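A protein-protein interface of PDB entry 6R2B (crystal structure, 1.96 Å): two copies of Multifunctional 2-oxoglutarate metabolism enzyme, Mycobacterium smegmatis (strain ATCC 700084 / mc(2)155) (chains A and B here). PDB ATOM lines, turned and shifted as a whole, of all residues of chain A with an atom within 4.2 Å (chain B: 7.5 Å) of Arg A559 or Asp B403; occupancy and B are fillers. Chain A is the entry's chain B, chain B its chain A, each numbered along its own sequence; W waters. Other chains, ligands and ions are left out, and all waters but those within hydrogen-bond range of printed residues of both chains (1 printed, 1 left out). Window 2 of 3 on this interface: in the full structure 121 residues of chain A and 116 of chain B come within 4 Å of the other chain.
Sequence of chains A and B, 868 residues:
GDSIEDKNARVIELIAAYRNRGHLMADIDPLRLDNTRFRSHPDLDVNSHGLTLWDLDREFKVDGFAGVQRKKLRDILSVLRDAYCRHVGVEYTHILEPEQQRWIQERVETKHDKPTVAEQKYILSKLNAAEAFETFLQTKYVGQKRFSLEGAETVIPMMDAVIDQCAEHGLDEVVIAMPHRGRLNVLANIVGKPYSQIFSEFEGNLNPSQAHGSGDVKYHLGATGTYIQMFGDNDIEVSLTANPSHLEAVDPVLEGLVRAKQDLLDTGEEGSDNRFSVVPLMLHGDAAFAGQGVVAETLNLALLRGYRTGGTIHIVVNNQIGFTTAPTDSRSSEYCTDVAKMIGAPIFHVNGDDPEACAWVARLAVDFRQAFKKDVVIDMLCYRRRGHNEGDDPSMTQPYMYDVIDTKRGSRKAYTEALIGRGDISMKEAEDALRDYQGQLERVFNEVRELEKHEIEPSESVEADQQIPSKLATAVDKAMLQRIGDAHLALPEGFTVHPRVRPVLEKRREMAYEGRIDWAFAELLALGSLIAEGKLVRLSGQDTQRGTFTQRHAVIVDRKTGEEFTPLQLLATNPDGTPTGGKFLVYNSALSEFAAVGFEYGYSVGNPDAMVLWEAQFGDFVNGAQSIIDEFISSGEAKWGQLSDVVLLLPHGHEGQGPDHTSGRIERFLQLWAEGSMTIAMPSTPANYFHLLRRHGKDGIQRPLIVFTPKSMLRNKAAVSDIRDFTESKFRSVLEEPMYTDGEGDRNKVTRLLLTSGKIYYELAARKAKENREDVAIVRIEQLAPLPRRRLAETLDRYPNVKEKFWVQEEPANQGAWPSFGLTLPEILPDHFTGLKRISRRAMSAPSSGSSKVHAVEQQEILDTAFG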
ATOM      1  N   THR A 496      10.398  19.617  23.505  1.00  0.00           N
ATOM      2  CA  THR A 496      10.778  18.232  23.689  1.00  0.00           C
ATOM      3  C   THR A 496      12.156  18.037  23.085  1.00  0.00           C
ATOM      4  O   THR A 496      12.326  18.082  21.881  1.00  0.00           O
ATOM      5  CB  THR A 496       9.719  17.267  23.120  1.00  0.00           C
ATOM      6  OG1 THR A 496       8.445  17.634  23.631  1.00  0.00           O
ATOM      7  CG2 THR A 496       9.995  15.831  23.502  1.00  0.00           C
ATOM      8  N   HIS A 498      15.340  15.777  22.033  1.00  0.00           N
ATOM      9  CA  HIS A 498      15.658  14.402  21.653  1.00  0.00           C
ATOM     10  C   HIS A 498      16.417  13.720  22.835  1.00  0.00           C
ATOM     11  O   HIS A 498      17.268  14.376  23.474  1.00  0.00           O
ATOM     12  CB  HIS A 498      16.502  14.407  20.394  1.00  0.00           C
ATOM     13  CG  HIS A 498      16.724  13.060  19.820  1.00  0.00           C
ATOM     14  ND1 HIS A 498      17.667  12.196  20.352  1.00  0.00           N
ATOM     15  CD2 HIS A 498      16.115  12.463  18.776  1.00  0.00           C
ATOM     16  CE1 HIS A 498      17.606  11.105  19.607  1.00  0.00           C
ATOM     17  NE2 HIS A 498      16.682  11.220  18.650  1.00  0.00           N
ATOM     18  N   VAL A 557      16.462  20.328  17.682  1.00  0.00           N
ATOM     19  CA  VAL A 557      15.150  20.191  17.051  1.00  0.00           C
ATOM     20  C   VAL A 557      14.213  19.443  17.971  1.00  0.00           C
ATOM     21  O   VAL A 557      14.549  18.359  18.475  1.00  0.00           O
ATOM     22  CB  VAL A 557      15.310  19.500  15.650  1.00  0.00           C
ATOM     23  CG1 VAL A 557      13.955  19.161  15.001  1.00  0.00           C
ATOM     24  CG2 VAL A 557      16.177  20.348  14.714  1.00  0.00           C
ATOM     25  N   ASP A 558      13.033  20.047  18.208  1.00  0.00           N
ATOM     26  CA  ASP A 558      11.972  19.477  19.030  1.00  0.00           C
ATOM     27  C   ASP A 558      11.583  18.097  18.485  1.00  0.00           C
ATOM     28  O   ASP A 558      11.210  17.968  17.307  1.00  0.00           O
ATOM     29  CB  ASP A 558      10.762  20.423  19.091  1.00  0.00           C
ATOM     30  CG  ASP A 558       9.723  19.997  20.100  1.00  0.00           C
ATOM     31  OD1 ASP A 558       9.075  18.949  19.888  1.00  0.00           O
ATOM     32  OD2 ASP A 558       9.551  20.706  21.099  1.00  0.00           O
ATOM     33  N   ARG A 559      11.709  17.067  19.345  1.00  0.00           N
ATOM     34  CA  ARG A 559      11.441  15.668  19.015  1.00  0.00           C
ATOM     35  C   ARG A 559       9.994  15.453  18.551  1.00  0.00           C
ATOM     36  O   ARG A 559       9.753  14.559  17.731  1.00  0.00           O
ATOM     37  CB  ARG A 559      11.781  14.736  20.220  1.00  0.00           C
ATOM     38  CG  ARG A 559      11.633  13.214  19.958  1.00  0.00           C
ATOM     39  CD  ARG A 559      12.533  12.746  18.824  1.00  0.00           C
ATOM     40  NE  ARG A 559      12.316  11.368  18.362  1.00  0.00           N
ATOM     41  CZ  ARG A 559      11.452  11.002  17.415  1.00  0.00           C
ATOM     42  NH1 ARG A 559      10.599  11.884  16.901  1.00  0.00           N
ATOM     43  NH2 ARG A 559      11.408   9.746  17.002  1.00  0.00           N
ATOM     44  N   LYS A 560       9.036  16.272  19.066  1.00  0.00           N
ATOM     45  CA  LYS A 560       7.617  16.138  18.751  1.00  0.00           C
ATOM     46  C   LYS A 560       7.119  17.034  17.598  1.00  0.00           C
ATOM     47  O   LYS A 560       6.239  16.597  16.857  1.00  0.00           O
ATOM     48  CB  LYS A 560       6.765  16.441  19.989  1.00  0.00           C
ATOM     49  CG  LYS A 560       6.751  15.337  21.035  1.00  0.00           C
ATOM     50  CD  LYS A 560       5.982  15.774  22.283  1.00  0.00           C
ATOM     51  CE  LYS A 560       6.010  14.708  23.339  1.00  0.00           C
ATOM     52  NZ  LYS A 560       5.288  15.129  24.564  1.00  0.00           N
ATOM     53  N   THR A 561       7.595  18.290  17.488  1.00  0.00           N
ATOM     54  CA  THR A 561       7.062  19.233  16.491  1.00  0.00           C
ATOM     55  C   THR A 561       8.037  19.652  15.358  1.00  0.00           C
ATOM     56  O   THR A 561       7.619  20.287  14.393  1.00  0.00           O
ATOM     57  CB  THR A 561       6.633  20.517  17.213  1.00  0.00           C
ATOM     58  OG1 THR A 561       7.802  21.151  17.751  1.00  0.00           O
ATOM     59  CG2 THR A 561       5.612  20.274  18.302  1.00  0.00           C
ATOM     60  N   ASP B 393      22.357   8.684  14.101  1.00  0.00           N
ATOM     61  CA  ASP B 393      20.939   8.764  14.505  1.00  0.00           C
ATOM     62  C   ASP B 393      20.279   9.960  13.772  1.00  0.00           C
ATOM     63  O   ASP B 393      20.600  11.114  14.061  1.00  0.00           O
ATOM     64  CB  ASP B 393      20.798   8.880  16.016  1.00  0.00           C
ATOM     65  CG  ASP B 393      19.389   8.775  16.554  1.00  0.00           C
ATOM     66  OD1 ASP B 393      18.438   8.914  15.764  1.00  0.00           O
ATOM     67  OD2 ASP B 393      19.241   8.520  17.751  1.00  0.00           O
ATOM     68  N   SER B 395      17.062  10.900  13.664  1.00  0.00           N
ATOM     69  CA  SER B 395      15.901  11.445  14.360  1.00  0.00           C
ATOM     70  C   SER B 395      16.263  12.698  15.182  1.00  0.00           C
ATOM     71  O   SER B 395      15.359  13.477  15.518  1.00  0.00           O
ATOM     72  CB  SER B 395      15.240  10.381  15.239  1.00  0.00           C
ATOM     73  OG  SER B 395      16.068   9.954  16.308  1.00  0.00           O
ATOM     74  N   MET B 396      17.559  12.904  15.519  1.00  0.00           N
ATOM     75  CA  MET B 396      17.945  14.153  16.197  1.00  0.00           C
ATOM     76  C   MET B 396      17.652  15.401  15.325  1.00  0.00           C
ATOM     77  O   MET B 396      17.260  16.437  15.852  1.00  0.00           O
ATOM     78  CB  MET B 396      19.430  14.170  16.604  1.00  0.00           C
ATOM     79  CG  MET B 396      19.816  13.165  17.654  1.00  0.00           C
ATOM     80  SD  MET B 396      21.619  13.100  17.951  1.00  0.00           S
ATOM     81  CE  MET B 396      22.142  12.675  16.384  1.00  0.00           C
ATOM     82  N   GLN B 398      15.960  15.101  11.845  1.00  0.00           N
ATOM     83  CA  GLN B 398      14.768  14.878  11.010  1.00  0.00           C
ATOM     84  C   GLN B 398      13.743  13.974  11.767  1.00  0.00           C
ATOM     85  O   GLN B 398      13.462  12.871  11.280  1.00  0.00           O
ATOM     86  CB  GLN B 398      15.163  14.268   9.654  1.00  0.00           C
ATOM     87  CG  GLN B 398      15.564  15.297   8.573  1.00  0.00           C
ATOM     88  CD  GLN B 398      16.943  15.863   8.814  1.00  0.00           C
ATOM     89  OE1 GLN B 398      17.866  15.172   9.264  1.00  0.00           O
ATOM     90  NE2 GLN B 398      17.123  17.120   8.491  1.00  0.00           N
ATOM     91  N   PRO B 399      13.190  14.401  12.949  1.00  0.00           N
ATOM     92  CA  PRO B 399      12.270  13.518  13.698  1.00  0.00           C
ATOM     93  C   PRO B 399      11.000  13.189  12.927  1.00  0.00           C
ATOM     94  O   PRO B 399      10.586  12.028  12.929  1.00  0.00           O
ATOM     95  CB  PRO B 399      11.948  14.309  14.963  1.00  0.00           C
ATOM     96  CG  PRO B 399      12.273  15.730  14.642  1.00  0.00           C
ATOM     97  CD  PRO B 399      13.425  15.659  13.687  1.00  0.00           C
ATOM     98  N   TYR B 400      10.418  14.184  12.227  1.00  0.00           N
ATOM     99  CA  TYR B 400       9.182  13.972  11.463  1.00  0.00           C
ATOM    100  C   TYR B 400       9.404  12.973  10.324  1.00  0.00           C
ATOM    101  O   TYR B 400       8.617  12.042  10.172  1.00  0.00           O
ATOM    102  CB  TYR B 400       8.614  15.292  10.931  1.00  0.00           C
ATOM    103  CG  TYR B 400       7.377  15.088  10.084  1.00  0.00           C
ATOM    104  CD1 TYR B 400       6.188  14.645  10.649  1.00  0.00           C
ATOM    105  CD2 TYR B 400       7.408  15.293   8.706  1.00  0.00           C
ATOM    106  CE1 TYR B 400       5.050  14.435   9.873  1.00  0.00           C
ATOM    107  CE2 TYR B 400       6.273  15.086   7.919  1.00  0.00           C
ATOM    108  CZ  TYR B 400       5.098  14.649   8.507  1.00  0.00           C
ATOM    109  OH  TYR B 400       3.970  14.446   7.750  1.00  0.00           O
ATOM    110  N   MET B 401      10.491  13.140   9.557  1.00  0.00           N
ATOM    111  CA  MET B 401      10.797  12.249   8.450  1.00  0.00           C
ATOM    112  C   MET B 401      10.975  10.811   8.956  1.00  0.00           C
ATOM    113  O   MET B 401      10.466   9.877   8.332  1.00  0.00           O
ATOM    114  CB  MET B 401      12.041  12.725   7.689  1.00  0.00           C
ATOM    115  CG  MET B 401      12.526  11.721   6.638  1.00  0.00           C
ATOM    116  SD  MET B 401      14.033  12.208   5.752  1.00  0.00           S
ATOM    117  CE  MET B 401      13.355  13.317   4.570  1.00  0.00           C
ATOM    118  N   TYR B 402      11.658  10.635  10.093  1.00  0.00           N
ATOM    119  CA  TYR B 402      11.905   9.276  10.539  1.00  0.00           C
ATOM    120  C   TYR B 402      10.698   8.695  11.241  1.00  0.00           C
ATOM    121  O   TYR B 402      10.527   7.483  11.146  1.00  0.00           O
ATOM    122  CB  TYR B 402      13.208   9.159  11.324  1.00  0.00           C
ATOM    123  CG  TYR B 402      14.293   9.070  10.278  1.00  0.00           C
ATOM    124  CD1 TYR B 402      14.801  10.224   9.675  1.00  0.00           C
ATOM    125  CD2 TYR B 402      14.619   7.847   9.697  1.00  0.00           C
ATOM    126  CE1 TYR B 402      15.649  10.154   8.573  1.00  0.00           C
ATOM    127  CE2 TYR B 402      15.510   7.764   8.633  1.00  0.00           C
ATOM    128  CZ  TYR B 402      16.018   8.920   8.070  1.00  0.00           C
ATOM    129  OH  TYR B 402      16.858   8.822   6.996  1.00  0.00           O
ATOM    130  N   ASP B 403       9.757   9.529  11.733  1.00  0.00           N
ATOM    131  CA  ASP B 403       8.502   9.002  12.282  1.00  0.00           C
ATOM    132  C   ASP B 403       7.644   8.395  11.134  1.00  0.00           C
ATOM    133  O   ASP B 403       6.996   7.378  11.339  1.00  0.00           O
ATOM    134  CB  ASP B 403       7.724  10.098  13.039  1.00  0.00           C
ATOM    135  CG  ASP B 403       8.323  10.511  14.375  1.00  0.00           C
ATOM    136  OD1 ASP B 403       8.962   9.659  15.034  1.00  0.00           O
ATOM    137  OD2 ASP B 403       8.138  11.677  14.767  1.00  0.00           O
ATOM    138  N   VAL B 404       7.705   8.989   9.913  1.00  0.00           N
ATOM    139  CA  VAL B 404       6.995   8.516   8.715  1.00  0.00           C
ATOM    140  C   VAL B 404       7.691   7.232   8.165  1.00  0.00           C
ATOM    141  O   VAL B 404       7.003   6.251   7.854  1.00  0.00           O
ATOM    142  CB  VAL B 404       6.900   9.642   7.627  1.00  0.00           C
ATOM    143  CG1 VAL B 404       6.298   9.123   6.320  1.00  0.00           C
ATOM    144  CG2 VAL B 404       6.107  10.852   8.139  1.00  0.00           C
ATOM    145  N   ILE B 405       9.050   7.250   8.041  1.00  0.00           N
ATOM    146  CA  ILE B 405       9.837   6.108   7.529  1.00  0.00           C
ATOM    147  C   ILE B 405       9.598   4.862   8.407  1.00  0.00           C
ATOM    148  O   ILE B 405       9.460   3.757   7.867  1.00  0.00           O
ATOM    149  CB  ILE B 405      11.356   6.451   7.379  1.00  0.00           C
ATOM    150  CG1 ILE B 405      11.560   7.470   6.228  1.00  0.00           C
ATOM    151  CG2 ILE B 405      12.225   5.192   7.133  1.00  0.00           C
ATOM    152  CD1 ILE B 405      12.984   8.173   6.173  1.00  0.00           C
ATOM    153  N   ASP B 406       9.524   5.049   9.735  1.00  0.00           N
ATOM    154  CA  ASP B 406       9.276   3.969  10.708  1.00  0.00           C
ATOM    155  C   ASP B 406       7.959   3.201  10.424  1.00  0.00           C
ATOM    156  O   ASP B 406       7.930   1.974  10.578  1.00  0.00           O
ATOM    157  CB  ASP B 406       9.261   4.539  12.141  1.00  0.00           C
ATOM    158  CG  ASP B 406      10.610   5.022  12.659  1.00  0.00           C
ATOM    159  OD1 ASP B 406      11.633   4.801  11.967  1.00  0.00           O
ATOM    160  OD2 ASP B 406      10.642   5.643  13.751  1.00  0.00           O
ATOM    161  N   THR B 407       6.888   3.918   9.984  1.00  0.00           N
ATOM    162  CA  THR B 407       5.564   3.342   9.665  1.00  0.00           C
ATOM    163  C   THR B 407       5.518   2.723   8.234  1.00  0.00           C
ATOM    164  O   THR B 407       4.462   2.262   7.787  1.00  0.00           O
ATOM    165  CB  THR B 407       4.444   4.425   9.769  1.00  0.00           C
ATOM    166  OG1 THR B 407       4.567   5.346   8.682  1.00  0.00           O
ATOM    167  CG2 THR B 407       4.422   5.163  11.108  1.00  0.00           C
ATOM    168  N   LYS B 408       6.655   2.700   7.542  1.00  0.00           N
ATOM    169  CA  LYS B 408       6.717   2.288   6.158  1.00  0.00           C
ATOM    170  C   LYS B 408       7.198   0.864   5.891  1.00  0.00           C
ATOM    171  O   LYS B 408       8.257   0.445   6.352  1.00  0.00           O
ATOM    172  CB  LYS B 408       7.646   3.260   5.418  1.00  0.00           C
ATOM    173  CG  LYS B 408       7.410   3.350   3.947  1.00  0.00           C
ATOM    174  CD  LYS B 408       6.362   4.388   3.607  1.00  0.00           C
ATOM    175  CE  LYS B 408       6.131   4.353   2.133  1.00  0.00           C
ATOM    176  NZ  LYS B 408       7.408   4.548   1.403  1.00  0.00           N
HETATM  177  O   HOH W   1      18.096  18.011  17.907  1.00  0.00           O
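The side-chain carboxylate of Asp B403 lies within salt-bridge range of the guanidinium group of Arg A559 (3.1 Å). A ring nitrogen (NE2) of His A498 sits at hydrogen-bond distance from the side-chain hydroxyl of Ser B395 (2.7 Å).
The side-chain carboxylate (OD1) of Asp A558 lies within hydrogen-bond range of the backbone NH (N) of Lys A560, at 2.8 Å. OD1 of Asp B393 lies within hydrogen-bond range of OG of Ser B395, 2.6 Å away. The backbone NH (N) of Thr A496 lies within hydrogen-bond range of the side-chain carboxylate (OD2) of Asp A558. The backbone carbonyl oxygen (O) of Thr A496 lies within hydrogen-bond range of the backbone NH (N) of Arg A559 (2.8 Å). OD1 of Asp A558 is in hydrogen-bond range of N of Thr A561, 2.9 Å away.
His A498 touches Asp B393 (CE1 to OD2, 3.6 Å). ND1 of His A498 touches CG of Met B396 (3.6 Å). Val A557 touches Met B396 (CB to O, 3.6 Å). CG1 of Val A557 touches CD of Pro B399, 3.8 Å away. O of Asp A558 touches CG of Pro B399 (3.6 Å). NH1 of Arg A559 touches CB of Pro B399, 3.4 Å away.
Of chain B, only Pro B399 (3.4 Å) and Asp B403 (3.1 Å) come within 4 Å of Arg A559. Asp B403 touches one residue of chain A. Printed residues of chain A within 4 Å of Ser B395: His A498. Of the printed residues of chain A, Asp B393 touches His A498. Printed residues of chain B within 4 Å of His A498: Asp B393, Ser B395 and Met B396. The nearest residue of chain B that does not touch Arg A559 is Ser B395 (4.3 Å).
Hydrophobic or aromatic side chains of chain B within 4 Å of the printed part of chain A: Met B396 and Pro B399. Of the 7 printed residues of chain A, 4 touch a printed residue of chain B. Hydrophobic or aromatic side chains of chain A that line the printed part of chain B: His A498 and Val A557. Among the printed residues, 8 pairs touch across the chains.
No position is printed for both chains. Of the 8 pairs that touch across the chains among the printed residues, none has its exchanged pair printed and touching as well.
Water W1 bridges O of Met B396 (2.7 Å) and N of Val A557 (2.8 Å).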
